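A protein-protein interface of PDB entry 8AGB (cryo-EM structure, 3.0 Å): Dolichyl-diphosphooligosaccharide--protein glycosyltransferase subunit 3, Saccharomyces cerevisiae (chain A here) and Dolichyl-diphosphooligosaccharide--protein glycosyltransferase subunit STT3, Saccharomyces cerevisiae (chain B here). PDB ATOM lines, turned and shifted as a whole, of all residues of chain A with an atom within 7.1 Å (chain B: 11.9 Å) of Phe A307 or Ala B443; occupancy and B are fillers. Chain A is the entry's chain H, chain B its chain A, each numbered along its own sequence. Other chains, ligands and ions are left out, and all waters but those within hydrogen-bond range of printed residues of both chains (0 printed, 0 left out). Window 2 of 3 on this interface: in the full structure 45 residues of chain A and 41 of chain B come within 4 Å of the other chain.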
ATOM      1  N   ARG A 295      -3.233 -26.472  -9.289  1.00  0.00           N
ATOM      2  CA  ARG A 295      -4.125 -27.622  -9.228  1.00  0.00           C
ATOM      3  C   ARG A 295      -5.190 -27.523 -10.311  1.00  0.00           C
ATOM      4  O   ARG A 295      -5.522 -28.520 -10.961  1.00  0.00           O
ATOM      5  CB  ARG A 295      -4.756 -27.721  -7.836  1.00  0.00           C
ATOM      6  CG  ARG A 295      -5.658 -28.932  -7.613  1.00  0.00           C
ATOM      7  CD  ARG A 295      -7.117 -28.631  -7.924  1.00  0.00           C
ATOM      8  NE  ARG A 295      -7.478 -27.261  -7.576  1.00  0.00           N
ATOM      9  CZ  ARG A 295      -8.580 -26.650  -7.999  1.00  0.00           C
ATOM     10  NH1 ARG A 295      -8.826 -25.397  -7.639  1.00  0.00           N
ATOM     11  NH2 ARG A 295      -9.433 -27.290  -8.788  1.00  0.00           N
ATOM     12  N   LYS A 303     -10.592 -34.553  -7.574  1.00  0.00           N
ATOM     13  CA  LYS A 303     -11.001 -35.589  -6.631  1.00  0.00           C
ATOM     14  C   LYS A 303     -10.274 -35.466  -5.299  1.00  0.00           C
ATOM     15  O   LYS A 303     -10.892 -35.619  -4.239  1.00  0.00           O
ATOM     16  CB  LYS A 303     -10.767 -36.978  -7.233  1.00  0.00           C
ATOM     17  CG  LYS A 303     -11.237 -38.126  -6.360  1.00  0.00           C
ATOM     18  CD  LYS A 303     -11.146 -39.448  -7.102  1.00  0.00           C
ATOM     19  CE  LYS A 303     -11.136 -40.621  -6.139  1.00  0.00           C
ATOM     20  NZ  LYS A 303     -10.020 -40.521  -5.160  1.00  0.00           N
ATOM     21  N   LYS A 304      -8.975 -35.189  -5.332  1.00  0.00           N
ATOM     22  CA  LYS A 304      -8.137 -35.064  -4.144  1.00  0.00           C
ATOM     23  C   LYS A 304      -7.335 -33.771  -4.202  1.00  0.00           C
ATOM     24  O   LYS A 304      -6.119 -33.751  -4.005  1.00  0.00           O
ATOM     25  CB  LYS A 304      -7.216 -36.272  -4.002  1.00  0.00           C
ATOM     26  CG  LYS A 304      -7.614 -37.229  -2.892  1.00  0.00           C
ATOM     27  CD  LYS A 304      -6.918 -38.569  -3.049  1.00  0.00           C
ATOM     28  CE  LYS A 304      -7.189 -39.477  -1.863  1.00  0.00           C
ATOM     29  NZ  LYS A 304      -6.470 -40.774  -1.988  1.00  0.00           N
ATOM     30  N   ALA A 305      -8.028 -32.667  -4.502  1.00  0.00           N
ATOM     31  CA  ALA A 305      -7.365 -31.373  -4.653  1.00  0.00           C
ATOM     32  C   ALA A 305      -6.542 -31.009  -3.424  1.00  0.00           C
ATOM     33  O   ALA A 305      -5.465 -30.412  -3.544  1.00  0.00           O
ATOM     34  CB  ALA A 305      -8.401 -30.288  -4.937  1.00  0.00           C
ATOM     35  N   TYR A 306      -7.040 -31.344  -2.231  1.00  0.00           N
ATOM     36  CA  TYR A 306      -6.298 -31.055  -1.009  1.00  0.00           C
ATOM     37  C   TYR A 306      -4.943 -31.749  -0.976  1.00  0.00           C
ATOM     38  O   TYR A 306      -4.059 -31.322  -0.227  1.00  0.00           O
ATOM     39  CB  TYR A 306      -7.125 -31.452   0.216  1.00  0.00           C
ATOM     40  CG  TYR A 306      -6.849 -32.848   0.724  1.00  0.00           C
ATOM     41  CD1 TYR A 306      -7.438 -33.952   0.125  1.00  0.00           C
ATOM     42  CD2 TYR A 306      -6.008 -33.061   1.806  1.00  0.00           C
ATOM     43  CE1 TYR A 306      -7.193 -35.229   0.585  1.00  0.00           C
ATOM     44  CE2 TYR A 306      -5.756 -34.334   2.272  1.00  0.00           C
ATOM     45  CZ  TYR A 306      -6.351 -35.415   1.660  1.00  0.00           C
ATOM     46  OH  TYR A 306      -6.103 -36.685   2.123  1.00  0.00           O
ATOM     47  N   PHE A 307      -4.759 -32.800  -1.771  1.00  0.00           N
ATOM     48  CA  PHE A 307      -3.488 -33.509  -1.839  1.00  0.00           C
ATOM     49  C   PHE A 307      -2.536 -32.879  -2.848  1.00  0.00           C
ATOM     50  O   PHE A 307      -1.337 -32.747  -2.571  1.00  0.00           O
ATOM     51  CB  PHE A 307      -3.731 -34.978  -2.193  1.00  0.00           C
ATOM     52  CG  PHE A 307      -2.550 -35.866  -1.943  1.00  0.00           C
ATOM     53  CD1 PHE A 307      -2.231 -36.268  -0.659  1.00  0.00           C
ATOM     54  CD2 PHE A 307      -1.765 -36.309  -2.993  1.00  0.00           C
ATOM     55  CE1 PHE A 307      -1.146 -37.089  -0.424  1.00  0.00           C
ATOM     56  CE2 PHE A 307      -0.679 -37.131  -2.766  1.00  0.00           C
ATOM     57  CZ  PHE A 307      -0.368 -37.522  -1.479  1.00  0.00           C
ATOM     58  N   ILE A 308      -3.051 -32.505  -4.022  1.00  0.00           N
ATOM     59  CA  ILE A 308      -2.238 -31.784  -4.995  1.00  0.00           C
ATOM     60  C   ILE A 308      -1.746 -30.473  -4.397  1.00  0.00           C
ATOM     61  O   ILE A 308      -0.594 -30.069  -4.607  1.00  0.00           O
ATOM     62  CB  ILE A 308      -3.040 -31.560  -6.290  1.00  0.00           C
ATOM     63  CG1 ILE A 308      -3.273 -32.888  -7.010  1.00  0.00           C
ATOM     64  CG2 ILE A 308      -2.326 -30.582  -7.203  1.00  0.00           C
ATOM     65  CD1 ILE A 308      -2.045 -33.765  -7.095  1.00  0.00           C
ATOM     66  N   ASP A 309      -2.609 -29.793  -3.636  1.00  0.00           N
ATOM     67  CA  ASP A 309      -2.206 -28.572  -2.944  1.00  0.00           C
ATOM     68  C   ASP A 309      -0.987 -28.825  -2.067  1.00  0.00           C
ATOM     69  O   ASP A 309       0.008 -28.092  -2.133  1.00  0.00           O
ATOM     70  CB  ASP A 309      -3.365 -28.033  -2.107  1.00  0.00           C
ATOM     71  CG  ASP A 309      -4.329 -27.184  -2.914  1.00  0.00           C
ATOM     72  OD1 ASP A 309      -4.736 -27.618  -4.012  1.00  0.00           O
ATOM     73  OD2 ASP A 309      -4.683 -26.080  -2.447  1.00  0.00           O
ATOM     74  N   ALA A 310      -1.057 -29.862  -1.231  1.00  0.00           N
ATOM     75  CA  ALA A 310       0.026 -30.153  -0.300  1.00  0.00           C
ATOM     76  C   ALA A 310       1.310 -30.509  -1.034  1.00  0.00           C
ATOM     77  O   ALA A 310       2.396 -30.034  -0.673  1.00  0.00           O
ATOM     78  CB  ALA A 310      -0.389 -31.293   0.631  1.00  0.00           C
ATOM     79  N   ILE A 311       1.208 -31.346  -2.068  1.00  0.00           N
ATOM     80  CA  ILE A 311       2.403 -31.763  -2.795  1.00  0.00           C
ATOM     81  C   ILE A 311       3.063 -30.564  -3.463  1.00  0.00           C
ATOM     82  O   ILE A 311       4.293 -30.413  -3.433  1.00  0.00           O
ATOM     83  CB  ILE A 311       2.057 -32.863  -3.813  1.00  0.00           C
ATOM     84  CG1 ILE A 311       1.547 -34.110  -3.091  1.00  0.00           C
ATOM     85  CG2 ILE A 311       3.267 -33.195  -4.666  1.00  0.00           C
ATOM     86  CD1 ILE A 311       2.644 -35.028  -2.599  1.00  0.00           C
ATOM     87  N   LEU A 312       2.258 -29.684  -4.062  1.00  0.00           N
ATOM     88  CA  LEU A 312       2.817 -28.517  -4.735  1.00  0.00           C
ATOM     89  C   LEU A 312       3.431 -27.540  -3.742  1.00  0.00           C
ATOM     90  O   LEU A 312       4.462 -26.927  -4.031  1.00  0.00           O
ATOM     91  CB  LEU A 312       1.738 -27.832  -5.572  1.00  0.00           C
ATOM     92  CG  LEU A 312       1.566 -28.284  -7.024  1.00  0.00           C
ATOM     93  CD1 LEU A 312       1.797 -29.774  -7.194  1.00  0.00           C
ATOM     94  CD2 LEU A 312       0.178 -27.920  -7.498  1.00  0.00           C
ATOM     95  N   ALA A 313       2.819 -27.383  -2.565  1.00  0.00           N
ATOM     96  CA  ALA A 313       3.422 -26.536  -1.540  1.00  0.00           C
ATOM     97  C   ALA A 313       4.775 -27.085  -1.104  1.00  0.00           C
ATOM     98  O   ALA A 313       5.750 -26.332  -0.966  1.00  0.00           O
ATOM     99  CB  ALA A 313       2.483 -26.409  -0.342  1.00  0.00           C
ATOM    100  N   SER A 314       4.848 -28.399  -0.881  1.00  0.00           N
ATOM    101  CA  SER A 314       6.112 -29.014  -0.488  1.00  0.00           C
ATOM    102  C   SER A 314       7.179 -28.818  -1.558  1.00  0.00           C
ATOM    103  O   SER A 314       8.334 -28.498  -1.246  1.00  0.00           O
ATOM    104  CB  SER A 314       5.897 -30.497  -0.206  1.00  0.00           C
ATOM    105  OG  SER A 314       4.781 -30.690   0.645  1.00  0.00           O
ATOM    106  N   ILE B 427      -1.188 -18.561   5.964  1.00  0.00           N
ATOM    107  CA  ILE B 427      -1.711 -19.734   5.291  1.00  0.00           C
ATOM    108  C   ILE B 427      -1.092 -21.008   5.845  1.00  0.00           C
ATOM    109  O   ILE B 427      -1.772 -22.029   5.963  1.00  0.00           O
ATOM    110  CB  ILE B 427      -1.498 -19.640   3.765  1.00  0.00           C
ATOM    111  CG1 ILE B 427      -1.890 -18.255   3.253  1.00  0.00           C
ATOM    112  CG2 ILE B 427      -2.299 -20.714   3.052  1.00  0.00           C
ATOM    113  CD1 ILE B 427      -2.089 -18.195   1.757  1.00  0.00           C
ATOM    114  N   TYR B 428       0.195 -20.972   6.193  1.00  0.00           N
ATOM    115  CA  TYR B 428       0.911 -22.195   6.529  1.00  0.00           C
ATOM    116  C   TYR B 428       1.203 -22.327   8.020  1.00  0.00           C
ATOM    117  O   TYR B 428       1.894 -23.266   8.425  1.00  0.00           O
ATOM    118  CB  TYR B 428       2.197 -22.294   5.711  1.00  0.00           C
ATOM    119  CG  TYR B 428       1.921 -22.430   4.234  1.00  0.00           C
ATOM    120  CD1 TYR B 428       1.360 -23.591   3.722  1.00  0.00           C
ATOM    121  CD2 TYR B 428       2.193 -21.394   3.356  1.00  0.00           C
ATOM    122  CE1 TYR B 428       1.094 -23.722   2.378  1.00  0.00           C
ATOM    123  CE2 TYR B 428       1.927 -21.516   2.008  1.00  0.00           C
ATOM    124  CZ  TYR B 428       1.379 -22.682   1.527  1.00  0.00           C
ATOM    125  OH  TYR B 428       1.113 -22.812   0.186  1.00  0.00           O
ATOM    126  N   ASP B 430      -1.765 -21.396  10.008  1.00  0.00           N
ATOM    127  CA  ASP B 430      -3.164 -21.484  10.419  1.00  0.00           C
ATOM    128  C   ASP B 430      -3.579 -22.946  10.328  1.00  0.00           C
ATOM    129  O   ASP B 430      -3.879 -23.450   9.245  1.00  0.00           O
ATOM    130  CB  ASP B 430      -4.032 -20.592   9.541  1.00  0.00           C
ATOM    131  CG  ASP B 430      -5.504 -20.881   9.694  1.00  0.00           C
ATOM    132  OD1 ASP B 430      -5.995 -20.833  10.837  1.00  0.00           O
ATOM    133  OD2 ASP B 430      -6.170 -21.154   8.674  1.00  0.00           O
ATOM    134  N   PHE B 431      -3.620 -23.626  11.475  1.00  0.00           N
ATOM    135  CA  PHE B 431      -3.849 -25.066  11.479  1.00  0.00           C
ATOM    136  C   PHE B 431      -5.323 -25.442  11.387  1.00  0.00           C
ATOM    137  O   PHE B 431      -5.644 -26.504  10.846  1.00  0.00           O
ATOM    138  CB  PHE B 431      -3.235 -25.684  12.735  1.00  0.00           C
ATOM    139  CG  PHE B 431      -1.735 -25.718  12.719  1.00  0.00           C
ATOM    140  CD1 PHE B 431      -1.057 -26.489  11.792  1.00  0.00           C
ATOM    141  CD2 PHE B 431      -1.003 -24.978  13.629  1.00  0.00           C
ATOM    142  CE1 PHE B 431       0.321 -26.522  11.776  1.00  0.00           C
ATOM    143  CE2 PHE B 431       0.376 -25.007  13.616  1.00  0.00           C
ATOM    144  CZ  PHE B 431       1.038 -25.780  12.689  1.00  0.00           C
ATOM    145  N   LYS B 432      -6.223 -24.613  11.909  1.00  0.00           N
ATOM    146  CA  LYS B 432      -7.652 -24.924  11.881  1.00  0.00           C
ATOM    147  C   LYS B 432      -8.152 -25.147  10.457  1.00  0.00           C
ATOM    148  O   LYS B 432      -8.570 -26.247  10.100  1.00  0.00           O
ATOM    149  CB  LYS B 432      -8.469 -23.815  12.547  1.00  0.00           C
ATOM    150  CG  LYS B 432      -8.386 -22.479  11.842  1.00  0.00           C
ATOM    151  CD  LYS B 432      -9.695 -21.718  11.925  1.00  0.00           C
ATOM    152  CE  LYS B 432      -9.513 -20.275  11.488  1.00  0.00           C
ATOM    153  NZ  LYS B 432      -8.617 -20.167  10.304  1.00  0.00           N
ATOM    154  N   ILE B 440      -8.827 -33.911   9.917  1.00  0.00           N
ATOM    155  CA  ILE B 440      -7.425 -33.620  10.187  1.00  0.00           C
ATOM    156  C   ILE B 440      -6.610 -33.624   8.893  1.00  0.00           C
ATOM    157  O   ILE B 440      -5.898 -32.659   8.607  1.00  0.00           O
ATOM    158  CB  ILE B 440      -6.842 -34.600  11.235  1.00  0.00           C
ATOM    159  CG1 ILE B 440      -5.345 -34.344  11.431  1.00  0.00           C
ATOM    160  CG2 ILE B 440      -7.146 -36.054  10.877  1.00  0.00           C
ATOM    161  CD1 ILE B 440      -5.028 -32.977  12.000  1.00  0.00           C
ATOM    162  N   LYS B 441      -6.726 -34.705   8.112  1.00  0.00           N
ATOM    163  CA  LYS B 441      -6.048 -34.852   6.828  1.00  0.00           C
ATOM    164  C   LYS B 441      -4.554 -34.591   6.978  1.00  0.00           C
ATOM    165  O   LYS B 441      -4.063 -33.528   6.574  1.00  0.00           O
ATOM    166  CB  LYS B 441      -6.669 -33.918   5.788  1.00  0.00           C
ATOM    167  CG  LYS B 441      -7.863 -34.531   5.072  1.00  0.00           C
ATOM    168  CD  LYS B 441      -8.789 -33.472   4.505  1.00  0.00           C
ATOM    169  CE  LYS B 441      -9.950 -34.107   3.758  1.00  0.00           C
ATOM    170  NZ  LYS B 441     -10.929 -33.095   3.275  1.00  0.00           N
ATOM    171  N   PRO B 442      -3.809 -35.534   7.573  1.00  0.00           N
ATOM    172  CA  PRO B 442      -2.386 -35.311   7.882  1.00  0.00           C
ATOM    173  C   PRO B 442      -1.522 -34.815   6.730  1.00  0.00           C
ATOM    174  O   PRO B 442      -0.438 -34.274   6.970  1.00  0.00           O
ATOM    175  CB  PRO B 442      -1.916 -36.694   8.354  1.00  0.00           C
ATOM    176  CG  PRO B 442      -2.966 -37.654   7.880  1.00  0.00           C
ATOM    177  CD  PRO B 442      -4.240 -36.892   7.932  1.00  0.00           C
ATOM    178  N   ALA B 443      -1.958 -35.016   5.485  1.00  0.00           N
ATOM    179  CA  ALA B 443      -1.193 -34.512   4.349  1.00  0.00           C
ATOM    180  C   ALA B 443      -1.034 -32.997   4.422  1.00  0.00           C
ATOM    181  O   ALA B 443       0.069 -32.463   4.240  1.00  0.00           O
ATOM    182  CB  ALA B 443      -1.867 -34.924   3.042  1.00  0.00           C
ATOM    183  N   ALA B 444      -2.136 -32.287   4.674  1.00  0.00           N
ATOM    184  CA  ALA B 444      -2.064 -30.839   4.830  1.00  0.00           C
ATOM    185  C   ALA B 444      -1.164 -30.459   5.997  1.00  0.00           C
ATOM    186  O   ALA B 444      -0.452 -29.450   5.941  1.00  0.00           O
ATOM    187  CB  ALA B 444      -3.464 -30.260   5.017  1.00  0.00           C
ATOM    188  N   LEU B 445      -1.179 -31.260   7.064  1.00  0.00           N
ATOM    189  CA  LEU B 445      -0.318 -30.982   8.208  1.00  0.00           C
ATOM    190  C   LEU B 445       1.152 -31.088   7.827  1.00  0.00           C
ATOM    191  O   LEU B 445       1.960 -30.234   8.205  1.00  0.00           O
ATOM    192  CB  LEU B 445      -0.646 -31.937   9.353  1.00  0.00           C
ATOM    193  CG  LEU B 445      -0.461 -31.389  10.766  1.00  0.00           C
ATOM    194  CD1 LEU B 445      -1.282 -30.130  10.962  1.00  0.00           C
ATOM    195  CD2 LEU B 445      -0.839 -32.443  11.792  1.00  0.00           C
ATOM    196  N   LEU B 446       1.515 -32.134   7.081  1.00  0.00           N
ATOM    197  CA  LEU B 446       2.889 -32.265   6.605  1.00  0.00           C
ATOM    198  C   LEU B 446       3.275 -31.093   5.714  1.00  0.00           C
ATOM    199  O   LEU B 446       4.383 -30.553   5.828  1.00  0.00           O
ATOM    200  CB  LEU B 446       3.061 -33.585   5.854  1.00  0.00           C
ATOM    201  CG  LEU B 446       3.584 -34.800   6.623  1.00  0.00           C
ATOM    202  CD1 LEU B 446       5.105 -34.789   6.668  1.00  0.00           C
ATOM    203  CD2 LEU B 446       3.005 -34.865   8.027  1.00  0.00           C
ATOM    204  N   ALA B 447       2.378 -30.695   4.810  1.00  0.00           N
ATOM    205  CA  ALA B 447       2.694 -29.604   3.894  1.00  0.00           C
ATOM    206  C   ALA B 447       2.845 -28.278   4.623  1.00  0.00           C
ATOM    207  O   ALA B 447       3.629 -27.423   4.199  1.00  0.00           O
ATOM    208  CB  ALA B 447       1.618 -29.483   2.823  1.00  0.00           C
ATOM    209  N   LYS B 448       2.096 -28.085   5.707  1.00  0.00           N
ATOM    210  CA  LYS B 448       2.247 -26.877   6.506  1.00  0.00           C
ATOM    211  C   LYS B 448       3.549 -26.907   7.292  1.00  0.00           C
ATOM    212  O   LYS B 448       4.266 -25.898   7.361  1.00  0.00           O
ATOM    213  CB  LYS B 448       1.054 -26.735   7.448  1.00  0.00           C
ATOM    214  CG  LYS B 448      -0.224 -26.314   6.757  1.00  0.00           C
ATOM    215  CD  LYS B 448      -1.431 -26.623   7.617  1.00  0.00           C
ATOM    216  CE  LYS B 448      -2.472 -25.533   7.514  1.00  0.00           C
ATOM    217  NZ  LYS B 448      -3.060 -25.454   6.153  1.00  0.00           N
ATOM    218  N   LEU B 449       3.855 -28.051   7.909  1.00  0.00           N
ATOM    219  CA  LEU B 449       5.068 -28.172   8.707  1.00  0.00           C
ATOM    220  C   LEU B 449       6.304 -27.935   7.853  1.00  0.00           C
ATOM    221  O   LEU B 449       7.222 -27.223   8.268  1.00  0.00           O
ATOM    222  CB  LEU B 449       5.130 -29.546   9.372  1.00  0.00           C
ATOM    223  CG  LEU B 449       4.139 -29.800  10.508  1.00  0.00           C
ATOM    224  CD1 LEU B 449       4.327 -31.193  11.080  1.00  0.00           C
ATOM    225  CD2 LEU B 449       4.291 -28.749  11.589  1.00  0.00           C
ATOM    226  N   ILE B 450       6.356 -28.546   6.667  1.00  0.00           N
ATOM    227  CA  ILE B 450       7.516 -28.389   5.789  1.00  0.00           C
ATOM    228  C   ILE B 450       7.829 -26.912   5.575  1.00  0.00           C
ATOM    229  O   ILE B 450       8.950 -26.449   5.823  1.00  0.00           O
ATOM    230  CB  ILE B 450       7.282 -29.117   4.454  1.00  0.00           C
ATOM    231  CG1 ILE B 450       7.533 -30.615   4.620  1.00  0.00           C
ATOM    232  CG2 ILE B 450       8.179 -28.549   3.371  1.00  0.00           C
ATOM    233  CD1 ILE B 450       7.566 -31.379   3.316  1.00  0.00           C
ATOM    234  N   VAL B 451       6.828 -26.144   5.141  1.00  0.00           N
ATOM    235  CA  VAL B 451       7.061 -24.755   4.754  1.00  0.00           C
ATOM    236  C   VAL B 451       7.364 -23.899   5.978  1.00  0.00           C
ATOM    237  O   VAL B 451       8.307 -23.093   5.977  1.00  0.00           O
ATOM    238  CB  VAL B 451       5.854 -24.211   3.971  1.00  0.00           C
ATOM    239  CG1 VAL B 451       6.023 -22.729   3.706  1.00  0.00           C
ATOM    240  CG2 VAL B 451       5.679 -24.977   2.676  1.00  0.00           C
ATOM    241  N   SER B 452       6.555 -24.041   7.032  1.00  0.00           N
ATOM    242  CA  SER B 452       6.779 -23.236   8.226  1.00  0.00           C
ATOM    243  C   SER B 452       8.154 -23.509   8.820  1.00  0.00           C
ATOM    244  O   SER B 452       8.855 -22.576   9.228  1.00  0.00           O
ATOM    245  CB  SER B 452       5.682 -23.500   9.254  1.00  0.00           C
ATOM    246  OG  SER B 452       5.417 -24.886   9.368  1.00  0.00           O
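O of Ala A310 is in hydrogen-bond range of OG of Ser A314, 2.8 Å away.
Along chain A the printed residues that touch a printed residue of chain B span positions 306 to 314.
Among the printed residues, 7 pairs touch across the chains.
Among the printed residues, no Asp or Glu carboxylate lies within 4 Å of a Lys or Arg side-chain nitrogen of the other chain.
Tyr A306 touches Lys B441.
CB of Ala B443 touches CD1 of Phe A307 (3.95 Å).
Ala A310 touches Ala B443.
Ala A310 touches Ala B447.
Ala A313 touches Tyr B428.
O of Ala A313 touches CG2 of Val B451 (3.9 Å).
Ile B450 touches Ser A314 (CD1 to OG, 3.9 Å).
Lys A303 touches none of the printed residues of chain B.
Lys A304 touches none of the printed residues of chain B.
No residue of chain B comes within 4 Å of Ala A305.
Phe A307 touches just one residue of chain B: Ala B443 (3.95 Å).
No residue of chain B comes within 4 Å of Ile A308.
No residue of chain B comes within 4 Å of Asp A309.
No residue of chain B comes within 4 Å of Ile A311.
Of the printed residues of chain A, Tyr B428 touches Ala A313.
Asp B430 touches none of the printed residues of chain A.
Of the printed residues of chain A, Lys B441 touches Tyr A306 (3.5 Å).
Printed residues of chain A within 4 Å of Ala B443: Phe A307 and Ala A310.
Printed residues of chain A within 4 Å of Ala B447: Ala A310.
Of the printed residues of chain A, Ile B450 touches Ser A314.
The nearest residue of chain B that does not touch Phe A307 is Ala B444 (6.7 Å).
The nearest printed residue of chain B that does not touch Ser A314 is Ala B447 (4.01 Å).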
